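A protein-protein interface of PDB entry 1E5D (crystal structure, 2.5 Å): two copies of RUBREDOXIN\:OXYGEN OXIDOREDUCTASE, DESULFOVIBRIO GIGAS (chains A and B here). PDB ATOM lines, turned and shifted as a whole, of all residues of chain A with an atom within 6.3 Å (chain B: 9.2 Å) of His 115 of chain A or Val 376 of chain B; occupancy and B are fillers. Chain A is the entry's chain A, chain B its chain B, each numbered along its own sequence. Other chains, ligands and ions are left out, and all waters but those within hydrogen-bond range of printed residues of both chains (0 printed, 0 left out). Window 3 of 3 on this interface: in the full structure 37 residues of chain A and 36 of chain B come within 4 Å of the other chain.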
ATOM      1  N   LEU A  82      18.571 -11.375   5.913  1.00  0.00           N
ATOM      2  CA  LEU A  82      17.179 -11.476   5.471  1.00  0.00           C
ATOM      3  C   LEU A  82      16.665 -10.232   4.780  1.00  0.00           C
ATOM      4  O   LEU A  82      15.631 -10.256   4.107  1.00  0.00           O
ATOM      5  CB  LEU A  82      16.295 -11.836   6.673  1.00  0.00           C
ATOM      6  CG  LEU A  82      16.490 -13.266   7.187  1.00  0.00           C
ATOM      7  CD1 LEU A  82      15.565 -13.553   8.358  1.00  0.00           C
ATOM      8  CD2 LEU A  82      16.270 -14.252   6.052  1.00  0.00           C
ATOM      9  N   MET A 110      22.738 -20.097   3.312  1.00  0.00           N
ATOM     10  CA  MET A 110      21.381 -20.289   2.795  1.00  0.00           C
ATOM     11  C   MET A 110      20.723 -21.481   3.473  1.00  0.00           C
ATOM     12  O   MET A 110      19.498 -21.533   3.629  1.00  0.00           O
ATOM     13  CB  MET A 110      21.412 -20.453   1.285  1.00  0.00           C
ATOM     14  CG  MET A 110      20.042 -20.413   0.625  1.00  0.00           C
ATOM     15  SD  MET A 110      20.211 -20.606  -1.166  1.00  0.00           S
ATOM     16  CE  MET A 110      20.944 -19.018  -1.576  1.00  0.00           C
ATOM     17  N   GLU A 111      21.506 -22.472   3.909  1.00  0.00           N
ATOM     18  CA  GLU A 111      20.833 -23.603   4.555  1.00  0.00           C
ATOM     19  C   GLU A 111      20.480 -23.299   6.010  1.00  0.00           C
ATOM     20  O   GLU A 111      19.387 -23.683   6.438  1.00  0.00           O
ATOM     21  CB  GLU A 111      21.659 -24.886   4.491  1.00  0.00           C
ATOM     22  CG  GLU A 111      22.973 -24.776   3.741  1.00  0.00           C
ATOM     23  CD  GLU A 111      23.804 -26.045   3.844  1.00  0.00           C
ATOM     24  OE1 GLU A 111      24.593 -26.157   4.807  1.00  0.00           O
ATOM     25  OE2 GLU A 111      23.665 -26.925   2.965  1.00  0.00           O
ATOM     26  N   SER A 112      21.358 -22.636   6.761  1.00  0.00           N
ATOM     27  CA  SER A 112      21.065 -22.367   8.171  1.00  0.00           C
ATOM     28  C   SER A 112      20.025 -21.269   8.358  1.00  0.00           C
ATOM     29  O   SER A 112      19.501 -21.068   9.450  1.00  0.00           O
ATOM     30  CB  SER A 112      22.353 -21.998   8.902  1.00  0.00           C
ATOM     31  OG  SER A 112      22.991 -20.908   8.257  1.00  0.00           O
ATOM     32  N   HIS A 113      19.712 -20.547   7.291  1.00  0.00           N
ATOM     33  CA  HIS A 113      18.608 -19.603   7.312  1.00  0.00           C
ATOM     34  C   HIS A 113      17.328 -20.266   6.795  1.00  0.00           C
ATOM     35  O   HIS A 113      16.255 -20.066   7.370  1.00  0.00           O
ATOM     36  CB  HIS A 113      18.879 -18.371   6.458  1.00  0.00           C
ATOM     37  CG  HIS A 113      19.672 -17.271   7.071  1.00  0.00           C
ATOM     38  ND1 HIS A 113      21.045 -17.244   7.125  1.00  0.00           N
ATOM     39  CD2 HIS A 113      19.268 -16.119   7.661  1.00  0.00           C
ATOM     40  CE1 HIS A 113      21.453 -16.141   7.719  1.00  0.00           C
ATOM     41  NE2 HIS A 113      20.386 -15.436   8.060  1.00  0.00           N
ATOM     42  N   PHE A 114      17.415 -21.030   5.700  1.00  0.00           N
ATOM     43  CA  PHE A 114      16.160 -21.453   5.070  1.00  0.00           C
ATOM     44  C   PHE A 114      15.915 -22.951   5.214  1.00  0.00           C
ATOM     45  O   PHE A 114      14.759 -23.360   5.090  1.00  0.00           O
ATOM     46  CB  PHE A 114      16.111 -21.070   3.587  1.00  0.00           C
ATOM     47  CG  PHE A 114      16.009 -19.562   3.387  1.00  0.00           C
ATOM     48  CD1 PHE A 114      14.832 -18.892   3.670  1.00  0.00           C
ATOM     49  CD2 PHE A 114      17.088 -18.829   2.922  1.00  0.00           C
ATOM     50  CE1 PHE A 114      14.727 -17.524   3.487  1.00  0.00           C
ATOM     51  CE2 PHE A 114      16.996 -17.467   2.729  1.00  0.00           C
ATOM     52  CZ  PHE A 114      15.808 -16.812   3.011  1.00  0.00           C
ATOM     53  N   HIS A 115      16.986 -23.691   5.475  1.00  0.00           N
ATOM     54  CA  HIS A 115      16.853 -25.128   5.688  1.00  0.00           C
ATOM     55  C   HIS A 115      16.070 -25.759   4.544  1.00  0.00           C
ATOM     56  O   HIS A 115      15.162 -26.560   4.755  1.00  0.00           O
ATOM     57  CB  HIS A 115      16.178 -25.373   7.038  1.00  0.00           C
ATOM     58  CG  HIS A 115      16.792 -24.593   8.162  1.00  0.00           C
ATOM     59  ND1 HIS A 115      18.076 -24.800   8.618  1.00  0.00           N
ATOM     60  CD2 HIS A 115      16.294 -23.594   8.927  1.00  0.00           C
ATOM     61  CE1 HIS A 115      18.345 -23.972   9.609  1.00  0.00           C
ATOM     62  NE2 HIS A 115      17.273 -23.228   9.815  1.00  0.00           N
ATOM     63  N   TYR A 116      16.414 -25.354   3.326  1.00  0.00           N
ATOM     64  CA  TYR A 116      15.704 -25.730   2.116  1.00  0.00           C
ATOM     65  C   TYR A 116      15.951 -27.176   1.714  1.00  0.00           C
ATOM     66  O   TYR A 116      17.019 -27.752   1.918  1.00  0.00           O
ATOM     67  CB  TYR A 116      16.113 -24.803   0.968  1.00  0.00           C
ATOM     68  CG  TYR A 116      17.571 -24.907   0.585  1.00  0.00           C
ATOM     69  CD1 TYR A 116      18.556 -24.223   1.284  1.00  0.00           C
ATOM     70  CD2 TYR A 116      17.962 -25.697  -0.488  1.00  0.00           C
ATOM     71  CE1 TYR A 116      19.894 -24.308   0.941  1.00  0.00           C
ATOM     72  CE2 TYR A 116      19.295 -25.788  -0.838  1.00  0.00           C
ATOM     73  CZ  TYR A 116      20.253 -25.100  -0.130  1.00  0.00           C
ATOM     74  OH  TYR A 116      21.575 -25.204  -0.489  1.00  0.00           O
ATOM     75  N   LYS A 117      14.919 -27.781   1.121  1.00  0.00           N
ATOM     76  CA  LYS A 117      15.096 -29.178   0.728  1.00  0.00           C
ATOM     77  C   LYS A 117      15.467 -29.280  -0.736  1.00  0.00           C
ATOM     78  O   LYS A 117      16.534 -29.774  -1.117  1.00  0.00           O
ATOM     79  CB  LYS A 117      13.839 -29.988   1.055  1.00  0.00           C
ATOM     80  CG  LYS A 117      14.150 -31.314   1.732  1.00  0.00           C
ATOM     81  CD  LYS A 117      14.012 -31.241   3.244  1.00  0.00           C
ATOM     82  CE  LYS A 117      14.102 -32.625   3.875  1.00  0.00           C
ATOM     83  NZ  LYS A 117      13.339 -32.710   5.153  1.00  0.00           N
ATOM     84  N   TRP B 263      17.368  -9.802  13.685  1.00  0.00           N
ATOM     85  CA  TRP B 263      16.570 -10.454  12.651  1.00  0.00           C
ATOM     86  C   TRP B 263      15.604 -11.485  13.202  1.00  0.00           C
ATOM     87  O   TRP B 263      15.046 -12.322  12.498  1.00  0.00           O
ATOM     88  CB  TRP B 263      17.511 -11.058  11.583  1.00  0.00           C
ATOM     89  CG  TRP B 263      17.947  -9.933  10.680  1.00  0.00           C
ATOM     90  CD1 TRP B 263      19.175  -9.345  10.630  1.00  0.00           C
ATOM     91  CD2 TRP B 263      17.133  -9.264   9.703  1.00  0.00           C
ATOM     92  NE1 TRP B 263      19.176  -8.352   9.679  1.00  0.00           N
ATOM     93  CE2 TRP B 263      17.940  -8.279   9.094  1.00  0.00           C
ATOM     94  CE3 TRP B 263      15.809  -9.402   9.284  1.00  0.00           C
ATOM     95  CZ2 TRP B 263      17.475  -7.436   8.090  1.00  0.00           C
ATOM     96  CZ3 TRP B 263      15.355  -8.559   8.288  1.00  0.00           C
ATOM     97  CH2 TRP B 263      16.174  -7.587   7.696  1.00  0.00           C
ATOM     98  N   HIS B 264      15.338 -11.398  14.497  1.00  0.00           N
ATOM     99  CA  HIS B 264      14.290 -12.126  15.181  1.00  0.00           C
ATOM    100  C   HIS B 264      14.594 -13.582  15.456  1.00  0.00           C
ATOM    101  O   HIS B 264      13.697 -14.298  15.919  1.00  0.00           O
ATOM    102  CB  HIS B 264      12.977 -12.062  14.363  1.00  0.00           C
ATOM    103  CG  HIS B 264      12.602 -10.619  14.194  1.00  0.00           C
ATOM    104  ND1 HIS B 264      12.210  -9.823  15.241  1.00  0.00           N
ATOM    105  CD2 HIS B 264      12.635  -9.847  13.085  1.00  0.00           C
ATOM    106  CE1 HIS B 264      11.975  -8.606  14.784  1.00  0.00           C
ATOM    107  NE2 HIS B 264      12.220  -8.598  13.484  1.00  0.00           N
ATOM    108  N   SER B 265      15.812 -14.062  15.195  1.00  0.00           N
ATOM    109  CA  SER B 265      15.979 -15.481  15.536  1.00  0.00           C
ATOM    110  C   SER B 265      16.056 -15.621  17.052  1.00  0.00           C
ATOM    111  O   SER B 265      15.447 -16.506  17.655  1.00  0.00           O
ATOM    112  CB  SER B 265      17.190 -16.063  14.821  1.00  0.00           C
ATOM    113  OG  SER B 265      16.887 -16.260  13.449  1.00  0.00           O
ATOM    114  N   THR B 266      16.816 -14.731  17.681  1.00  0.00           N
ATOM    115  CA  THR B 266      16.919 -14.780  19.141  1.00  0.00           C
ATOM    116  C   THR B 266      15.570 -14.449  19.752  1.00  0.00           C
ATOM    117  O   THR B 266      15.256 -14.791  20.888  1.00  0.00           O
ATOM    118  CB  THR B 266      17.998 -13.804  19.636  1.00  0.00           C
ATOM    119  OG1 THR B 266      19.258 -14.189  19.064  1.00  0.00           O
ATOM    120  CG2 THR B 266      18.146 -13.860  21.150  1.00  0.00           C
ATOM    121  N   LYS B 268      12.614 -15.547  18.484  1.00  0.00           N
ATOM    122  CA  LYS B 268      11.929 -16.826  18.386  1.00  0.00           C
ATOM    123  C   LYS B 268      12.372 -17.780  19.492  1.00  0.00           C
ATOM    124  O   LYS B 268      11.550 -18.403  20.161  1.00  0.00           O
ATOM    125  CB  LYS B 268      12.180 -17.483  17.030  1.00  0.00           C
ATOM    126  CG  LYS B 268      11.603 -16.747  15.835  1.00  0.00           C
ATOM    127  CD  LYS B 268      12.366 -17.114  14.567  1.00  0.00           C
ATOM    128  CE  LYS B 268      12.062 -16.158  13.424  1.00  0.00           C
ATOM    129  NZ  LYS B 268      12.527 -16.718  12.122  1.00  0.00           N
ATOM    130  N   MET B 269      13.677 -17.906  19.703  1.00  0.00           N
ATOM    131  CA  MET B 269      14.173 -18.700  20.826  1.00  0.00           C
ATOM    132  C   MET B 269      13.561 -18.201  22.124  1.00  0.00           C
ATOM    133  O   MET B 269      13.074 -18.973  22.956  1.00  0.00           O
ATOM    134  CB  MET B 269      15.702 -18.646  20.834  1.00  0.00           C
ATOM    135  CG  MET B 269      16.313 -19.261  19.582  1.00  0.00           C
ATOM    136  SD  MET B 269      18.031 -18.804  19.290  1.00  0.00           S
ATOM    137  CE  MET B 269      18.834 -19.514  20.721  1.00  0.00           C
ATOM    138  N   GLY B 343      21.220 -17.629  22.249  1.00  0.00           N
ATOM    139  CA  GLY B 343      21.341 -16.714  21.136  1.00  0.00           C
ATOM    140  C   GLY B 343      21.557 -17.423  19.807  1.00  0.00           C
ATOM    141  O   GLY B 343      21.840 -18.616  19.722  1.00  0.00           O
ATOM    142  N   SER B 344      21.420 -16.627  18.754  1.00  0.00           N
ATOM    143  CA  SER B 344      21.701 -17.025  17.391  1.00  0.00           C
ATOM    144  C   SER B 344      23.030 -16.413  16.968  1.00  0.00           C
ATOM    145  O   SER B 344      23.381 -15.306  17.381  1.00  0.00           O
ATOM    146  CB  SER B 344      20.587 -16.581  16.445  1.00  0.00           C
ATOM    147  OG  SER B 344      20.821 -17.087  15.142  1.00  0.00           O
ATOM    148  N   PHE B 345      23.761 -17.159  16.145  1.00  0.00           N
ATOM    149  CA  PHE B 345      24.995 -16.603  15.600  1.00  0.00           C
ATOM    150  C   PHE B 345      25.116 -17.032  14.140  1.00  0.00           C
ATOM    151  O   PHE B 345      24.434 -17.971  13.723  1.00  0.00           O
ATOM    152  CB  PHE B 345      26.208 -17.053  16.413  1.00  0.00           C
ATOM    153  CG  PHE B 345      26.572 -18.499  16.104  1.00  0.00           C
ATOM    154  CD1 PHE B 345      25.827 -19.516  16.659  1.00  0.00           C
ATOM    155  CD2 PHE B 345      27.636 -18.813  15.276  1.00  0.00           C
ATOM    156  CE1 PHE B 345      26.128 -20.833  16.378  1.00  0.00           C
ATOM    157  CE2 PHE B 345      27.942 -20.127  14.982  1.00  0.00           C
ATOM    158  CZ  PHE B 345      27.182 -21.134  15.537  1.00  0.00           C
ATOM    159  N   GLY B 346      25.999 -16.333  13.441  1.00  0.00           N
ATOM    160  CA  GLY B 346      26.314 -16.622  12.057  1.00  0.00           C
ATOM    161  C   GLY B 346      27.646 -17.333  11.894  1.00  0.00           C
ATOM    162  O   GLY B 346      27.748 -18.255  11.082  1.00  0.00           O
ATOM    163  N   LYS B 372      23.051 -22.341  21.769  1.00  0.00           N
ATOM    164  CA  LYS B 372      23.458 -21.488  20.659  1.00  0.00           C
ATOM    165  C   LYS B 372      23.031 -22.136  19.345  1.00  0.00           C
ATOM    166  O   LYS B 372      23.133 -23.353  19.189  1.00  0.00           O
ATOM    167  CB  LYS B 372      24.966 -21.251  20.695  1.00  0.00           C
ATOM    168  CG  LYS B 372      25.776 -22.507  20.413  1.00  0.00           C
ATOM    169  CD  LYS B 372      27.253 -22.280  20.709  1.00  0.00           C
ATOM    170  CE  LYS B 372      27.720 -20.986  20.062  1.00  0.00           C
ATOM    171  NZ  LYS B 372      27.584 -19.818  20.976  1.00  0.00           N
ATOM    172  N   VAL B 373      22.550 -21.325  18.422  1.00  0.00           N
ATOM    173  CA  VAL B 373      22.040 -21.737  17.130  1.00  0.00           C
ATOM    174  C   VAL B 373      22.623 -20.894  16.000  1.00  0.00           C
ATOM    175  O   VAL B 373      22.727 -19.672  16.140  1.00  0.00           O
ATOM    176  CB  VAL B 373      20.509 -21.605  17.097  1.00  0.00           C
ATOM    177  CG1 VAL B 373      19.882 -22.321  18.283  1.00  0.00           C
ATOM    178  CG2 VAL B 373      20.133 -20.129  17.089  1.00  0.00           C
ATOM    179  N   LYS B 374      22.984 -21.560  14.904  1.00  0.00           N
ATOM    180  CA  LYS B 374      23.486 -20.870  13.721  1.00  0.00           C
ATOM    181  C   LYS B 374      22.300 -20.288  12.954  1.00  0.00           C
ATOM    182  O   LYS B 374      21.502 -21.056  12.426  1.00  0.00           O
ATOM    183  CB  LYS B 374      24.298 -21.798  12.832  1.00  0.00           C
ATOM    184  CG  LYS B 374      25.550 -21.184  12.224  1.00  0.00           C
ATOM    185  CD  LYS B 374      25.833 -21.737  10.838  1.00  0.00           C
ATOM    186  CE  LYS B 374      26.777 -22.925  10.853  1.00  0.00           C
ATOM    187  NZ  LYS B 374      28.210 -22.521  10.922  1.00  0.00           N
ATOM    188  N   ASN B 375      22.214 -18.964  12.931  1.00  0.00           N
ATOM    189  CA  ASN B 375      21.119 -18.257  12.269  1.00  0.00           C
ATOM    190  C   ASN B 375      19.741 -18.741  12.719  1.00  0.00           C
ATOM    191  O   ASN B 375      19.440 -18.680  13.914  1.00  0.00           O
ATOM    192  CB  ASN B 375      21.260 -18.370  10.742  1.00  0.00           C
ATOM    193  CG  ASN B 375      22.608 -17.824  10.303  1.00  0.00           C
ATOM    194  OD1 ASN B 375      23.367 -18.474   9.586  1.00  0.00           O
ATOM    195  ND2 ASN B 375      22.916 -16.601  10.732  1.00  0.00           N
ATOM    196  N   VAL B 376      18.910 -19.201  11.795  1.00  0.00           N
ATOM    197  CA  VAL B 376      17.501 -19.491  12.015  1.00  0.00           C
ATOM    198  C   VAL B 376      17.274 -20.884  12.586  1.00  0.00           C
ATOM    199  O   VAL B 376      17.589 -21.910  11.993  1.00  0.00           O
ATOM    200  CB  VAL B 376      16.703 -19.335  10.704  1.00  0.00           C
ATOM    201  CG1 VAL B 376      15.251 -19.752  10.863  1.00  0.00           C
ATOM    202  CG2 VAL B 376      16.785 -17.890  10.231  1.00  0.00           C
ATOM    203  N   PRO B 377      16.705 -20.892  13.788  1.00  0.00           N
ATOM    204  CA  PRO B 377      16.496 -22.135  14.524  1.00  0.00           C
ATOM    205  C   PRO B 377      15.478 -23.059  13.858  1.00  0.00           C
ATOM    206  O   PRO B 377      14.558 -22.616  13.173  1.00  0.00           O
ATOM    207  CB  PRO B 377      15.969 -21.657  15.884  1.00  0.00           C
ATOM    208  CG  PRO B 377      15.473 -20.274  15.678  1.00  0.00           C
ATOM    209  CD  PRO B 377      16.240 -19.703  14.521  1.00  0.00           C
ATOM    210  N   THR B 378      15.675 -24.348  14.093  1.00  0.00           N
ATOM    211  CA  THR B 378      14.788 -25.406  13.633  1.00  0.00           C
ATOM    212  C   THR B 378      14.261 -26.235  14.807  1.00  0.00           C
ATOM    213  O   THR B 378      14.813 -26.115  15.903  1.00  0.00           O
ATOM    214  CB  THR B 378      15.476 -26.371  12.653  1.00  0.00           C
ATOM    215  OG1 THR B 378      15.150 -27.707  13.057  1.00  0.00           O
ATOM    216  CG2 THR B 378      16.986 -26.237  12.716  1.00  0.00           C
ATOM    217  N   HIS B 379      13.236 -27.030  14.547  1.00  0.00           N
ATOM    218  CA  HIS B 379      12.525 -27.842  15.519  1.00  0.00           C
ATOM    219  C   HIS B 379      13.480 -28.491  16.513  1.00  0.00           C
ATOM    220  O   HIS B 379      13.251 -28.551  17.721  1.00  0.00           O
ATOM    221  CB  HIS B 379      11.708 -28.933  14.821  1.00  0.00           C
ATOM    222  CG  HIS B 379      11.196 -29.994  15.745  1.00  0.00           C
ATOM    223  ND1 HIS B 379      10.012 -29.859  16.441  1.00  0.00           N
ATOM    224  CD2 HIS B 379      11.670 -31.215  16.093  1.00  0.00           C
ATOM    225  CE1 HIS B 379       9.788 -30.935  17.175  1.00  0.00           C
ATOM    226  NE2 HIS B 379      10.787 -31.778  16.983  1.00  0.00           N
ATOM    227  N   ALA B 380      14.597 -28.979  15.971  1.00  0.00           N
ATOM    228  CA  ALA B 380      15.597 -29.544  16.868  1.00  0.00           C
ATOM    229  C   ALA B 380      16.038 -28.485  17.875  1.00  0.00           C
ATOM    230  O   ALA B 380      16.005 -28.726  19.081  1.00  0.00           O
ATOM    231  CB  ALA B 380      16.780 -30.089  16.090  1.00  0.00           C
ATOM    232  N   ASP B 381      16.435 -27.317  17.377  1.00  0.00           N
ATOM    233  CA  ASP B 381      16.870 -26.241  18.262  1.00  0.00           C
ATOM    234  C   ASP B 381      15.812 -25.944  19.317  1.00  0.00           C
ATOM    235  O   ASP B 381      16.121 -25.656  20.474  1.00  0.00           O
ATOM    236  CB  ASP B 381      17.173 -24.984  17.446  1.00  0.00           C
ATOM    237  CG  ASP B 381      18.235 -25.283  16.397  1.00  0.00           C
ATOM    238  OD1 ASP B 381      19.313 -25.779  16.798  1.00  0.00           O
ATOM    239  OD2 ASP B 381      17.955 -25.015  15.206  1.00  0.00           O
ATOM    240  N   TYR B 382      14.551 -26.026  18.887  1.00  0.00           N
ATOM    241  CA  TYR B 382      13.471 -25.790  19.834  1.00  0.00           C
ATOM    242  C   TYR B 382      13.486 -26.835  20.943  1.00  0.00           C
ATOM    243  O   TYR B 382      13.234 -26.502  22.103  1.00  0.00           O
ATOM    244  CB  TYR B 382      12.120 -25.772  19.103  1.00  0.00           C
ATOM    245  CG  TYR B 382      12.040 -24.524  18.244  1.00  0.00           C
ATOM    246  CD1 TYR B 382      12.746 -23.393  18.638  1.00  0.00           C
ATOM    247  CD2 TYR B 382      11.293 -24.481  17.081  1.00  0.00           C
ATOM    248  CE1 TYR B 382      12.701 -22.237  17.884  1.00  0.00           C
ATOM    249  CE2 TYR B 382      11.251 -23.323  16.326  1.00  0.00           C
ATOM    250  CZ  TYR B 382      11.952 -22.209  16.728  1.00  0.00           C
ATOM    251  OH  TYR B 382      11.902 -21.062  15.968  1.00  0.00           O
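The side-chain amide oxygen of Asn 375 of chain B is in hydrogen-bond range of the side-chain hydroxyl of Ser 112 of chain A (2.8 Å). The backbone carbonyl oxygen of Val 376 of chain B lies within hydrogen-bond range of a ring nitrogen (NE2) of His 115 of chain A (2.6 Å). O of Ser 112 of chain A sits at hydrogen-bond distance from N of Val 376 of chain B, 3.1 Å away.
O of Phe 345 of chain B lies within hydrogen-bond range of N of Asn 375 of chain B (2.6 Å). O of Ser 112 of chain A sits at hydrogen-bond distance from NE2 of His 115 of chain A (3.1 Å). The backbone carbonyl oxygen (O) of Glu 111 of chain A lies within hydrogen-bond range of a ring nitrogen (ND1) of His 115 of chain A. O of Asn 375 of chain B sits at hydrogen-bond distance from OG of Ser 344 of chain B, 2.4 Å away.
Among the printed residues, pairs that only touch across the chains: His 113 of chain A with Asn 375 of chain B (3.3 Å), His 113 of chain A with Val 376 of chain B (3.4 Å), Ser 112 of chain A with Lys 374 of chain B (3.6 Å) and Leu 82 of chain A with Trp 263 of chain B (3.6 Å).
Of the printed residues of chain B, Leu 82 of chain A touches Trp 263. Printed residues of chain B within 4 Å of Ser 112 of chain A: Lys 374 (3.6 Å), Asn 375 (2.8 Å) and Val 376 (3.1 Å). Of the printed residues of chain B, His 115 of chain A touches Val 376 (2.6 Å). Printed residues of chain A within 4 Å of Trp 263 of chain B: Leu 82. Lys 268 of chain B touches none of the printed residues of chain A. Ser 344 of chain B touches none of the printed residues of chain A. Of the printed residues of chain A, Lys 374 of chain B touches Ser 112. Printed residues of chain A within 4 Å of Asn 375 of chain B: Ser 112 (2.8 Å) and His 113 (3.3 Å). The nearest residue of chain B that does not touch His 115 of chain A is Thr 378 of chain B (4.1 Å). The nearest printed residue of chain B that does not touch Leu 82 of chain A is Val 376 of chain B (4.9 Å).
Of the 21 printed residues of chain B, 4 touch a printed residue of chain A. Hydrophobic or aromatic side chains of chain B within 4 Å of the printed part of chain A: Trp 263 and Val 376. Hydrophobic or aromatic side chains of chain A that line the printed part of chain B: Leu 82, His 113 and His 115.
No position is printed for both chains. Of the 7 pairs that touch across the chains among the printed residues, none has its exchanged pair printed and touching as well.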
